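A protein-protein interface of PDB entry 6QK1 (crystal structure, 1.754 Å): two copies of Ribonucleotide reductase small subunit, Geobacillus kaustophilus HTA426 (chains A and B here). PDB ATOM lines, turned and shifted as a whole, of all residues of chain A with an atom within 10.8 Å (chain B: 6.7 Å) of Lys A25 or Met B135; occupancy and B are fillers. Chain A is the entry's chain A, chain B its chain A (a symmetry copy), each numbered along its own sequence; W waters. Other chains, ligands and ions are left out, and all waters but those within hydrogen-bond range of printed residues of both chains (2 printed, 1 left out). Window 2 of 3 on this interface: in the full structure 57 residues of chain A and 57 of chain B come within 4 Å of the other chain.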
ATOM      1  N   HIS A  17     -17.987 -42.537  -2.965  1.00  0.00           N
ATOM      2  CA  HIS A  17     -17.591 -41.164  -2.665  1.00  0.00           C
ATOM      3  C   HIS A  17     -16.178 -40.833  -3.161  1.00  0.00           C
ATOM      4  O   HIS A  17     -15.305 -41.700  -3.253  1.00  0.00           O
ATOM      5  CB  HIS A  17     -17.677 -40.945  -1.144  1.00  0.00           C
ATOM      6  CG  HIS A  17     -19.057 -41.145  -0.564  1.00  0.00           C
ATOM      7  ND1 HIS A  17     -20.158 -41.481  -1.332  1.00  0.00           N
ATOM      8  CD2 HIS A  17     -19.506 -41.051   0.714  1.00  0.00           C
ATOM      9  CE1 HIS A  17     -21.221 -41.586  -0.551  1.00  0.00           C
ATOM     10  NE2 HIS A  17     -20.855 -41.328   0.693  1.00  0.00           N
ATOM     11  N   HIS A  18     -15.947 -39.550  -3.464  1.00  0.00           N
ATOM     12  CA  HIS A  18     -14.586 -39.033  -3.592  1.00  0.00           C
ATOM     13  C   HIS A  18     -14.021 -38.721  -2.200  1.00  0.00           C
ATOM     14  O   HIS A  18     -14.700 -38.110  -1.380  1.00  0.00           O
ATOM     15  CB  HIS A  18     -14.563 -37.763  -4.458  1.00  0.00           C
ATOM     16  CG  HIS A  18     -15.065 -37.955  -5.855  1.00  0.00           C
ATOM     17  ND1 HIS A  18     -14.368 -38.672  -6.808  1.00  0.00           N
ATOM     18  CD2 HIS A  18     -16.182 -37.494  -6.475  1.00  0.00           C
ATOM     19  CE1 HIS A  18     -15.048 -38.667  -7.945  1.00  0.00           C
ATOM     20  NE2 HIS A  18     -16.149 -37.955  -7.772  1.00  0.00           N
ATOM     21  N   ASP A  19     -12.791 -39.151  -1.917  1.00  0.00           N
ATOM     22  CA  ASP A  19     -12.180 -38.811  -0.627  1.00  0.00           C
ATOM     23  C   ASP A  19     -11.471 -37.456  -0.657  1.00  0.00           C
ATOM     24  O   ASP A  19     -11.193 -36.891   0.405  1.00  0.00           O
ATOM     25  CB  ASP A  19     -11.207 -39.920  -0.173  1.00  0.00           C
ATOM     26  CG  ASP A  19     -11.936 -41.174   0.401  1.00  0.00           C
ATOM     27  OD1 ASP A  19     -13.048 -41.044   0.968  1.00  0.00           O
ATOM     28  OD2 ASP A  19     -11.392 -42.299   0.293  1.00  0.00           O
ATOM     29  N   GLY A  20     -11.202 -36.920  -1.838  1.00  0.00           N
ATOM     30  CA  GLY A  20     -10.602 -35.608  -1.997  1.00  0.00           C
ATOM     31  C   GLY A  20     -10.223 -35.455  -3.455  1.00  0.00           C
ATOM     32  O   GLY A  20     -10.409 -36.370  -4.256  1.00  0.00           O
ATOM     33  N   PHE A  21      -9.654 -34.294  -3.787  1.00  0.00           N
ATOM     34  CA  PHE A  21      -9.317 -33.989  -5.167  1.00  0.00           C
ATOM     35  C   PHE A  21      -7.880 -33.498  -5.261  1.00  0.00           C
ATOM     36  O   PHE A  21      -7.471 -32.583  -4.530  1.00  0.00           O
ATOM     37  CB  PHE A  21     -10.307 -32.964  -5.723  1.00  0.00           C
ATOM     38  CG  PHE A  21     -11.718 -33.460  -5.699  1.00  0.00           C
ATOM     39  CD1 PHE A  21     -12.163 -34.300  -6.707  1.00  0.00           C
ATOM     40  CD2 PHE A  21     -12.596 -33.127  -4.669  1.00  0.00           C
ATOM     41  CE1 PHE A  21     -13.452 -34.817  -6.698  1.00  0.00           C
ATOM     42  CE2 PHE A  21     -13.907 -33.636  -4.658  1.00  0.00           C
ATOM     43  CZ  PHE A  21     -14.331 -34.473  -5.672  1.00  0.00           C
ATOM     44  N   GLN A  22      -7.143 -34.102  -6.196  1.00  0.00           N
ATOM     45  CA  GLN A  22      -5.727 -33.800  -6.374  1.00  0.00           C
ATOM     46  C   GLN A  22      -5.498 -32.320  -6.677  1.00  0.00           C
ATOM     47  O   GLN A  22      -4.496 -31.731  -6.233  1.00  0.00           O
ATOM     48  CB  GLN A  22      -5.172 -34.700  -7.492  1.00  0.00           C
ATOM     49  CG  GLN A  22      -3.698 -34.503  -7.774  1.00  0.00           C
ATOM     50  CD  GLN A  22      -3.193 -35.385  -8.875  1.00  0.00           C
ATOM     51  OE1 GLN A  22      -3.643 -36.541  -9.034  1.00  0.00           O
ATOM     52  NE2 GLN A  22      -2.255 -34.858  -9.656  1.00  0.00           N
ATOM     53  N   THR A  23      -6.399 -31.681  -7.441  1.00  0.00           N
ATOM     54  CA  THR A  23      -6.131 -30.302  -7.835  1.00  0.00           C
ATOM     55  C   THR A  23      -6.645 -29.290  -6.789  1.00  0.00           C
ATOM     56  O   THR A  23      -6.537 -28.080  -6.997  1.00  0.00           O
ATOM     57  CB  THR A  23      -6.706 -30.036  -9.229  1.00  0.00           C
ATOM     58  OG1 THR A  23      -8.113 -30.285  -9.220  1.00  0.00           O
ATOM     59  CG2 THR A  23      -6.005 -30.964 -10.238  1.00  0.00           C
ATOM     60  N   VAL A  24      -7.132 -29.787  -5.652  1.00  0.00           N
ATOM     61  CA  VAL A  24      -7.434 -28.984  -4.471  1.00  0.00           C
ATOM     62  C   VAL A  24      -6.345 -29.144  -3.413  1.00  0.00           C
ATOM     63  O   VAL A  24      -5.877 -28.161  -2.835  1.00  0.00           O
ATOM     64  CB  VAL A  24      -8.818 -29.400  -3.917  1.00  0.00           C
ATOM     65  CG1 VAL A  24      -9.116 -28.760  -2.591  1.00  0.00           C
ATOM     66  CG2 VAL A  24      -9.919 -29.022  -4.889  1.00  0.00           C
ATOM     67  N   LYS A  25      -5.918 -30.383  -3.183  1.00  0.00           N
ATOM     68  CA  LYS A  25      -4.832 -30.646  -2.234  1.00  0.00           C
ATOM     69  C   LYS A  25      -3.487 -30.227  -2.786  1.00  0.00           C
ATOM     70  O   LYS A  25      -2.596 -29.826  -2.024  1.00  0.00           O
ATOM     71  CB  LYS A  25      -4.811 -32.138  -1.884  1.00  0.00           C
ATOM     72  CG  LYS A  25      -6.026 -32.555  -1.039  1.00  0.00           C
ATOM     73  CD  LYS A  25      -6.590 -33.925  -1.403  1.00  0.00           C
ATOM     74  CE  LYS A  25      -6.106 -35.023  -0.470  1.00  0.00           C
ATOM     75  NZ  LYS A  25      -6.410 -36.395  -1.016  1.00  0.00           N
ATOM     76  N   ALA A  26      -3.325 -30.298  -4.107  1.00  0.00           N
ATOM     77  CA  ALA A  26      -2.044 -30.031  -4.751  1.00  0.00           C
ATOM     78  C   ALA A  26      -2.269 -29.497  -6.166  1.00  0.00           C
ATOM     79  O   ALA A  26      -3.033 -28.542  -6.348  1.00  0.00           O
ATOM     80  CB  ALA A  26      -1.194 -31.310  -4.713  1.00  0.00           C
ATOM     81  N   THR A  27      -1.578 -30.052  -7.156  1.00  0.00           N
ATOM     82  CA  THR A  27      -1.777 -29.689  -8.555  1.00  0.00           C
ATOM     83  C   THR A  27      -1.667 -30.953  -9.397  1.00  0.00           C
ATOM     84  O   THR A  27      -1.344 -32.041  -8.903  1.00  0.00           O
ATOM     85  CB  THR A  27      -0.754 -28.648  -9.069  1.00  0.00           C
ATOM     86  OG1 THR A  27       0.546 -29.266  -9.199  1.00  0.00           O
ATOM     87  CG2 THR A  27      -0.653 -27.408  -8.142  1.00  0.00           C
ATOM     88  N   ILE A  28      -1.932 -30.801 -10.698  1.00  0.00           N
ATOM     89  CA  ILE A  28      -1.587 -31.811 -11.678  1.00  0.00           C
ATOM     90  C   ILE A  28      -0.098 -32.109 -11.532  1.00  0.00           C
ATOM     91  O   ILE A  28       0.685 -31.198 -11.237  1.00  0.00           O
ATOM     92  CB  ILE A  28      -1.916 -31.263 -13.080  1.00  0.00           C
ATOM     93  CG1 ILE A  28      -3.438 -31.087 -13.230  1.00  0.00           C
ATOM     94  CG2 ILE A  28      -1.299 -32.112 -14.162  1.00  0.00           C
ATOM     95  CD1 ILE A  28      -3.824 -30.527 -14.586  1.00  0.00           C
ATOM     96  N   ASP A  29       0.313 -33.362 -11.747  1.00  0.00           N
ATOM     97  CA  ASP A  29       1.737 -33.681 -11.858  1.00  0.00           C
ATOM     98  C   ASP A  29       2.201 -33.307 -13.273  1.00  0.00           C
ATOM     99  O   ASP A  29       2.074 -34.089 -14.223  1.00  0.00           O
ATOM    100  CB  ASP A  29       2.002 -35.145 -11.544  1.00  0.00           C
ATOM    101  CG  ASP A  29       3.493 -35.519 -11.679  1.00  0.00           C
ATOM    102  OD1 ASP A  29       4.350 -34.632 -11.962  1.00  0.00           O
ATOM    103  OD2 ASP A  29       3.786 -36.723 -11.566  1.00  0.00           O
ATOM    104  N   TRP A  30       2.731 -32.091 -13.390  1.00  0.00           N
ATOM    105  CA  TRP A  30       3.079 -31.490 -14.672  1.00  0.00           C
ATOM    106  C   TRP A  30       4.146 -32.279 -15.413  1.00  0.00           C
ATOM    107  O   TRP A  30       4.237 -32.175 -16.653  1.00  0.00           O
ATOM    108  CB  TRP A  30       3.537 -30.035 -14.458  1.00  0.00           C
ATOM    109  CG  TRP A  30       2.628 -29.224 -13.617  1.00  0.00           C
ATOM    110  CD1 TRP A  30       2.858 -28.766 -12.342  1.00  0.00           C
ATOM    111  CD2 TRP A  30       1.313 -28.793 -13.965  1.00  0.00           C
ATOM    112  NE1 TRP A  30       1.783 -28.067 -11.894  1.00  0.00           N
ATOM    113  CE2 TRP A  30       0.815 -28.055 -12.876  1.00  0.00           C
ATOM    114  CE3 TRP A  30       0.519 -28.942 -15.107  1.00  0.00           C
ATOM    115  CZ2 TRP A  30      -0.467 -27.475 -12.874  1.00  0.00           C
ATOM    116  CZ3 TRP A  30      -0.774 -28.368 -15.103  1.00  0.00           C
ATOM    117  CH2 TRP A  30      -1.241 -27.634 -14.004  1.00  0.00           C
ATOM    118  N   GLY A 101      -7.094 -43.151  -9.208  1.00  0.00           N
ATOM    119  CA  GLY A 101      -6.513 -41.853  -8.931  1.00  0.00           C
ATOM    120  C   GLY A 101      -5.465 -41.379  -9.912  1.00  0.00           C
ATOM    121  O   GLY A 101      -4.744 -40.419  -9.618  1.00  0.00           O
ATOM    122  N   LEU A 103      -4.910 -39.310 -12.359  1.00  0.00           N
ATOM    123  CA  LEU A 103      -5.592 -38.163 -12.982  1.00  0.00           C
ATOM    124  C   LEU A 103      -4.978 -37.805 -14.337  1.00  0.00           C
ATOM    125  O   LEU A 103      -5.699 -37.463 -15.295  1.00  0.00           O
ATOM    126  CB  LEU A 103      -5.565 -36.950 -12.060  1.00  0.00           C
ATOM    127  CG  LEU A 103      -6.246 -35.671 -12.614  1.00  0.00           C
ATOM    128  CD1 LEU A 103      -7.716 -35.846 -12.940  1.00  0.00           C
ATOM    129  CD2 LEU A 103      -6.080 -34.574 -11.601  1.00  0.00           C
ATOM    130  N   PHE B  61      -1.759 -11.414  -7.638  1.00  0.00           N
ATOM    131  CA  PHE B  61      -1.875 -12.194  -6.412  1.00  0.00           C
ATOM    132  C   PHE B  61      -0.780 -11.811  -5.417  1.00  0.00           C
ATOM    133  O   PHE B  61      -1.047 -11.664  -4.219  1.00  0.00           O
ATOM    134  CB  PHE B  61      -1.815 -13.690  -6.734  1.00  0.00           C
ATOM    135  CG  PHE B  61      -2.327 -14.550  -5.632  1.00  0.00           C
ATOM    136  CD1 PHE B  61      -3.679 -14.708  -5.454  1.00  0.00           C
ATOM    137  CD2 PHE B  61      -1.458 -15.169  -4.747  1.00  0.00           C
ATOM    138  CE1 PHE B  61      -4.182 -15.492  -4.441  1.00  0.00           C
ATOM    139  CE2 PHE B  61      -1.959 -15.966  -3.717  1.00  0.00           C
ATOM    140  CZ  PHE B  61      -3.321 -16.121  -3.563  1.00  0.00           C
ATOM    141  N   LYS B  69      -5.538 -11.890  -0.424  1.00  0.00           N
ATOM    142  CA  LYS B  69      -5.259 -13.223  -0.970  1.00  0.00           C
ATOM    143  C   LYS B  69      -6.373 -14.216  -0.643  1.00  0.00           C
ATOM    144  O   LYS B  69      -6.941 -14.850  -1.539  1.00  0.00           O
ATOM    145  CB  LYS B  69      -3.918 -13.759  -0.436  1.00  0.00           C
ATOM    146  CG  LYS B  69      -2.680 -13.290  -1.191  1.00  0.00           C
ATOM    147  CD  LYS B  69      -1.437 -14.085  -0.756  1.00  0.00           C
ATOM    148  CE  LYS B  69      -0.227 -13.726  -1.572  1.00  0.00           C
ATOM    149  NZ  LYS B  69       0.321 -12.383  -1.263  1.00  0.00           N
ATOM    150  N   ILE B  70      -6.714 -14.351   0.637  1.00  0.00           N
ATOM    151  CA  ILE B  70      -7.712 -15.335   1.050  1.00  0.00           C
ATOM    152  C   ILE B  70      -9.010 -15.165   0.278  1.00  0.00           C
ATOM    153  O   ILE B  70      -9.666 -16.152  -0.084  1.00  0.00           O
ATOM    154  CB  ILE B  70      -7.958 -15.238   2.568  1.00  0.00           C
ATOM    155  CG1 ILE B  70      -7.157 -16.318   3.295  1.00  0.00           C
ATOM    156  CG2 ILE B  70      -9.470 -15.329   2.919  1.00  0.00           C
ATOM    157  CD1 ILE B  70      -7.561 -17.728   2.952  1.00  0.00           C
ATOM    158  N   LEU B  73      -9.747 -17.525  -2.661  1.00  0.00           N
ATOM    159  CA  LEU B  73      -9.431 -18.944  -2.645  1.00  0.00           C
ATOM    160  C   LEU B  73     -10.659 -19.840  -2.466  1.00  0.00           C
ATOM    161  O   LEU B  73     -10.649 -20.948  -3.017  1.00  0.00           O
ATOM    162  CB  LEU B  73      -8.394 -19.247  -1.557  1.00  0.00           C
ATOM    163  CG  LEU B  73      -7.025 -18.556  -1.724  1.00  0.00           C
ATOM    164  CD1 LEU B  73      -6.033 -19.045  -0.694  1.00  0.00           C
ATOM    165  CD2 LEU B  73      -6.458 -18.754  -3.117  1.00  0.00           C
ATOM    166  N   GLU B  84     -12.733 -31.384 -11.291  1.00  0.00           N
ATOM    167  CA  GLU B  84     -12.137 -32.708 -11.195  1.00  0.00           C
ATOM    168  C   GLU B  84     -13.210 -33.786 -11.001  1.00  0.00           C
ATOM    169  O   GLU B  84     -13.188 -34.819 -11.683  1.00  0.00           O
ATOM    170  CB  GLU B  84     -11.099 -32.698 -10.062  1.00  0.00           C
ATOM    171  CG  GLU B  84     -10.244 -33.957 -10.050  1.00  0.00           C
ATOM    172  CD  GLU B  84      -9.093 -33.880  -9.020  1.00  0.00           C
ATOM    173  OE1 GLU B  84      -8.505 -32.784  -8.838  1.00  0.00           O
ATOM    174  OE2 GLU B  84      -8.811 -34.921  -8.407  1.00  0.00           O
ATOM    175  N   GLN B 127      -3.516 -21.918 -10.092  1.00  0.00           N
ATOM    176  CA  GLN B 127      -2.982 -22.156  -8.746  1.00  0.00           C
ATOM    177  C   GLN B 127      -1.461 -22.289  -8.777  1.00  0.00           C
ATOM    178  O   GLN B 127      -0.750 -21.674  -7.971  1.00  0.00           O
ATOM    179  CB  GLN B 127      -3.616 -23.405  -8.146  1.00  0.00           C
ATOM    180  CG  GLN B 127      -5.080 -23.269  -7.763  1.00  0.00           C
ATOM    181  CD  GLN B 127      -5.605 -24.488  -7.020  1.00  0.00           C
ATOM    182  OE1 GLN B 127      -6.705 -25.032  -7.331  1.00  0.00           O
ATOM    183  NE2 GLN B 127      -4.830 -24.947  -6.046  1.00  0.00           N
ATOM    184  N   GLY B 131       1.191 -19.269  -7.098  1.00  0.00           N
ATOM    185  CA  GLY B 131       1.971 -19.711  -5.965  1.00  0.00           C
ATOM    186  C   GLY B 131       1.228 -20.438  -4.872  1.00  0.00           C
ATOM    187  O   GLY B 131       1.785 -20.561  -3.776  1.00  0.00           O
ATOM    188  N   ILE B 132       0.012 -20.951  -5.124  1.00  0.00           N
ATOM    189  CA  ILE B 132      -0.748 -21.677  -4.108  1.00  0.00           C
ATOM    190  C   ILE B 132      -0.949 -23.150  -4.466  1.00  0.00           C
ATOM    191  O   ILE B 132      -1.747 -23.819  -3.817  1.00  0.00           O
ATOM    192  CB  ILE B 132      -2.101 -21.024  -3.808  1.00  0.00           C
ATOM    193  CG1 ILE B 132      -3.016 -21.090  -5.025  1.00  0.00           C
ATOM    194  CG2 ILE B 132      -1.919 -19.604  -3.339  1.00  0.00           C
ATOM    195  CD1 ILE B 132      -4.411 -20.586  -4.748  1.00  0.00           C
ATOM    196  N   GLY B 133      -0.182 -23.691  -5.420  1.00  0.00           N
ATOM    197  CA  GLY B 133      -0.306 -25.111  -5.745  1.00  0.00           C
ATOM    198  C   GLY B 133      -0.101 -26.018  -4.544  1.00  0.00           C
ATOM    199  O   GLY B 133      -0.758 -27.055  -4.416  1.00  0.00           O
ATOM    200  N   GLN B 134       0.837 -25.656  -3.662  1.00  0.00           N
ATOM    201  CA  GLN B 134       1.152 -26.441  -2.471  1.00  0.00           C
ATOM    202  C   GLN B 134       0.140 -26.262  -1.335  1.00  0.00           C
ATOM    203  O   GLN B 134       0.179 -27.027  -0.367  1.00  0.00           O
ATOM    204  CB  GLN B 134       2.572 -26.063  -1.985  1.00  0.00           C
ATOM    205  CG  GLN B 134       2.689 -24.728  -1.304  1.00  0.00           C
ATOM    206  CD  GLN B 134       2.556 -23.537  -2.207  1.00  0.00           C
ATOM    207  OE1 GLN B 134       2.756 -23.629  -3.416  1.00  0.00           O
ATOM    208  NE2 GLN B 134       2.222 -22.384  -1.619  1.00  0.00           N
ATOM    209  N   MET B 135      -0.739 -25.270  -1.409  1.00  0.00           N
ATOM    210  CA  MET B 135      -1.772 -25.079  -0.406  1.00  0.00           C
ATOM    211  C   MET B 135      -2.943 -26.037  -0.602  1.00  0.00           C
ATOM    212  O   MET B 135      -3.452 -26.198  -1.716  1.00  0.00           O
ATOM    213  CB  MET B 135      -2.241 -23.630  -0.471  1.00  0.00           C
ATOM    214  CG  MET B 135      -3.201 -23.176   0.612  1.00  0.00           C
ATOM    215  SD  MET B 135      -3.686 -21.431   0.381  1.00  0.00           S
ATOM    216  CE  MET B 135      -2.107 -20.578   0.239  1.00  0.00           C
ATOM    217  N   ASP B 136      -3.408 -26.642   0.496  1.00  0.00           N
ATOM    218  CA  ASP B 136      -4.550 -27.560   0.452  1.00  0.00           C
ATOM    219  C   ASP B 136      -5.834 -26.751   0.638  1.00  0.00           C
ATOM    220  O   ASP B 136      -6.170 -26.347   1.751  1.00  0.00           O
ATOM    221  CB  ASP B 136      -4.432 -28.661   1.507  1.00  0.00           C
ATOM    222  CG  ASP B 136      -5.593 -29.663   1.455  1.00  0.00           C
ATOM    223  OD1 ASP B 136      -6.552 -29.464   0.669  1.00  0.00           O
ATOM    224  OD2 ASP B 136      -5.551 -30.670   2.206  1.00  0.00           O
ATOM    225  N   LEU B 137      -6.573 -26.542  -0.454  1.00  0.00           N
ATOM    226  CA  LEU B 137      -7.766 -25.705  -0.434  1.00  0.00           C
ATOM    227  C   LEU B 137      -9.031 -26.459  -0.009  1.00  0.00           C
ATOM    228  O   LEU B 137     -10.118 -25.885  -0.076  1.00  0.00           O
ATOM    229  CB  LEU B 137      -7.971 -25.063  -1.818  1.00  0.00           C
ATOM    230  CG  LEU B 137      -6.834 -24.186  -2.379  1.00  0.00           C
ATOM    231  CD1 LEU B 137      -7.194 -23.566  -3.742  1.00  0.00           C
ATOM    232  CD2 LEU B 137      -6.423 -23.099  -1.432  1.00  0.00           C
ATOM    233  N   SER B 138      -8.906 -27.713   0.451  1.00  0.00           N
ATOM    234  CA  SER B 138     -10.044 -28.501   0.938  1.00  0.00           C
ATOM    235  C   SER B 138     -10.726 -27.860   2.142  1.00  0.00           C
ATOM    236  O   SER B 138     -11.892 -28.161   2.432  1.00  0.00           O
ATOM    237  CB  SER B 138      -9.580 -29.923   1.361  1.00  0.00           C
ATOM    238  OG  SER B 138      -9.026 -30.670   0.289  1.00  0.00           O
ATOM    239  N   VAL B 139      -9.994 -27.037   2.891  1.00  0.00           N
ATOM    240  CA  VAL B 139     -10.558 -26.339   4.039  1.00  0.00           C
ATOM    241  C   VAL B 139     -11.759 -25.462   3.693  1.00  0.00           C
ATOM    242  O   VAL B 139     -12.528 -25.102   4.591  1.00  0.00           O
ATOM    243  CB  VAL B 139      -9.441 -25.498   4.708  1.00  0.00           C
ATOM    244  CG1 VAL B 139      -8.834 -24.518   3.723  1.00  0.00           C
ATOM    245  CG2 VAL B 139      -9.978 -24.773   5.944  1.00  0.00           C
ATOM    246  N   PHE B 140     -11.959 -25.114   2.419  1.00  0.00           N
ATOM    247  CA  PHE B 140     -13.102 -24.297   2.021  1.00  0.00           C
ATOM    248  C   PHE B 140     -14.251 -25.125   1.444  1.00  0.00           C
ATOM    249  O   PHE B 140     -15.153 -24.561   0.824  1.00  0.00           O
ATOM    250  CB  PHE B 140     -12.677 -23.227   1.006  1.00  0.00           C
ATOM    251  CG  PHE B 140     -11.618 -22.287   1.529  1.00  0.00           C
ATOM    252  CD1 PHE B 140     -11.877 -21.509   2.635  1.00  0.00           C
ATOM    253  CD2 PHE B 140     -10.362 -22.206   0.926  1.00  0.00           C
ATOM    254  CE1 PHE B 140     -10.917 -20.641   3.131  1.00  0.00           C
ATOM    255  CE2 PHE B 140      -9.401 -21.337   1.423  1.00  0.00           C
ATOM    256  CZ  PHE B 140      -9.687 -20.563   2.540  1.00  0.00           C
HETATM  257  O   HOH W   1     -10.147 -32.342  -1.639  1.00  0.00           O
HETATM  258  O   HOH W   2      -4.285 -27.290  -8.474  1.00  0.00           O
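The side-chain carboxylate of Glu B84 is in hydrogen-bond range of the backbone NH of Gln A22 (2.9 Å). OE1 of Glu B84 sits at hydrogen-bond distance from OG1 of Thr A23. The backbone carbonyl oxygen of Thr A23 sits close to the side-chain amide oxygen of Gln B127 (3.1 Å). The backbone NH (N) of Leu B137 is in hydrogen-bond range of the backbone carbonyl oxygen (O) of Val A24. The backbone carbonyl oxygen (O) of Met B135 sits close to the backbone carbonyl oxygen (O) of Val A24 (3.3 Å). The backbone carbonyl oxygen of Gly B133 lies close to the backbone carbonyl oxygen of Ala A26 (3.3 Å).
NE2 of Gln A22 lies within hydrogen-bond range of O of Thr A27, 3.1 Å away. OG1 of Thr A27 is in hydrogen-bond range of NE1 of Trp A30 (3.2 Å). N of Ile B132 lies within hydrogen-bond range of O of Gln B127, 3.0 Å away. O of Gln B127 lies within hydrogen-bond range of N of Gly B133 (3.3 Å). OD1 of Asp B136 lies within hydrogen-bond range of OG of Ser B138, 2.8 Å away.
CA of Phe A21 touches OE2 of Glu B84 (3.4 Å). O of Val A24 touches CA of Asp B136 (3.6 Å). Val A24 touches Ser B138. O of Met B135 touches O of Lys A25 (3.7 Å). OD1 of Asp B136 touches CG of Lys A25, 3.6 Å away. CG of Lys A25 touches OG of Ser B138, at 3.8 Å. Thr A27 touches Gly B133.
Asp A19 touches none of the printed residues of chain B. Of the printed residues of chain B, Val A24 touches Met B135 (3.3 Å), Asp B136 (3.6 Å), Leu B137 (3.0 Å) and Ser B138 (3.2 Å). Of chain B, only Met B135, Asp B136 and Ser B138 come within 4 Å of Lys A25. Printed residues of chain A within 4 Å of Glu B84: Phe A21, Gln A22 and Thr A23. Of the printed residues of chain A, Gln B127 touches Thr A23. Ile B132 touches none of the printed residues of chain A. Of the printed residues of chain A, Gly B133 touches Ala A26 (3.3 Å) and Thr A27 (3.3 Å). Gln B134 touches none of the printed residues of chain A. Of chain A, only Val A24 (3.3 Å) and Lys A25 (3.7 Å) come within 4 Å of Met B135. Of the printed residues of chain A, Leu B137 touches Val A24 (3.0 Å). Printed residues of chain A within 4 Å of Ser B138: Val A24 and Lys A25. The nearest residue of chain B that does not touch Lys A25 is Gly B133 (4.1 Å). The nearest printed residue of chain A that does not touch Leu B137 is Lys A25 (4.8 Å).
Of the 16 printed residues of chain A, 7 touch a printed residue of chain B. Printed residues of chain A that touch a printed residue of chain B: Phe A21, Gln A22, Thr A23, Val A24, Lys A25, Ala A26 and Thr A27. Along chain A the printed residues that touch a printed residue of chain B span positions 21 to 27. Among the printed residues, 13 pairs touch across the chains. Among the printed residues, no Asp or Glu carboxylate lies within 4 Å of a Lys or Arg side-chain nitrogen of the other chain.
No position is printed for both chains. Of the 13 pairs that touch across the chains among the printed residues, none has its exchanged pair printed and touching as well.
Water W2 lies within hydrogen-bond range of O of Ala A26 (2.8 Å), O of Thr A23 (2.8 Å) and NE2 of Gln B127 (3.4 Å). Water W1 bridges the side-chain hydroxyl of Ser B138 (2.8 Å) and the backbone NH of Phe A21 (2.9 Å).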
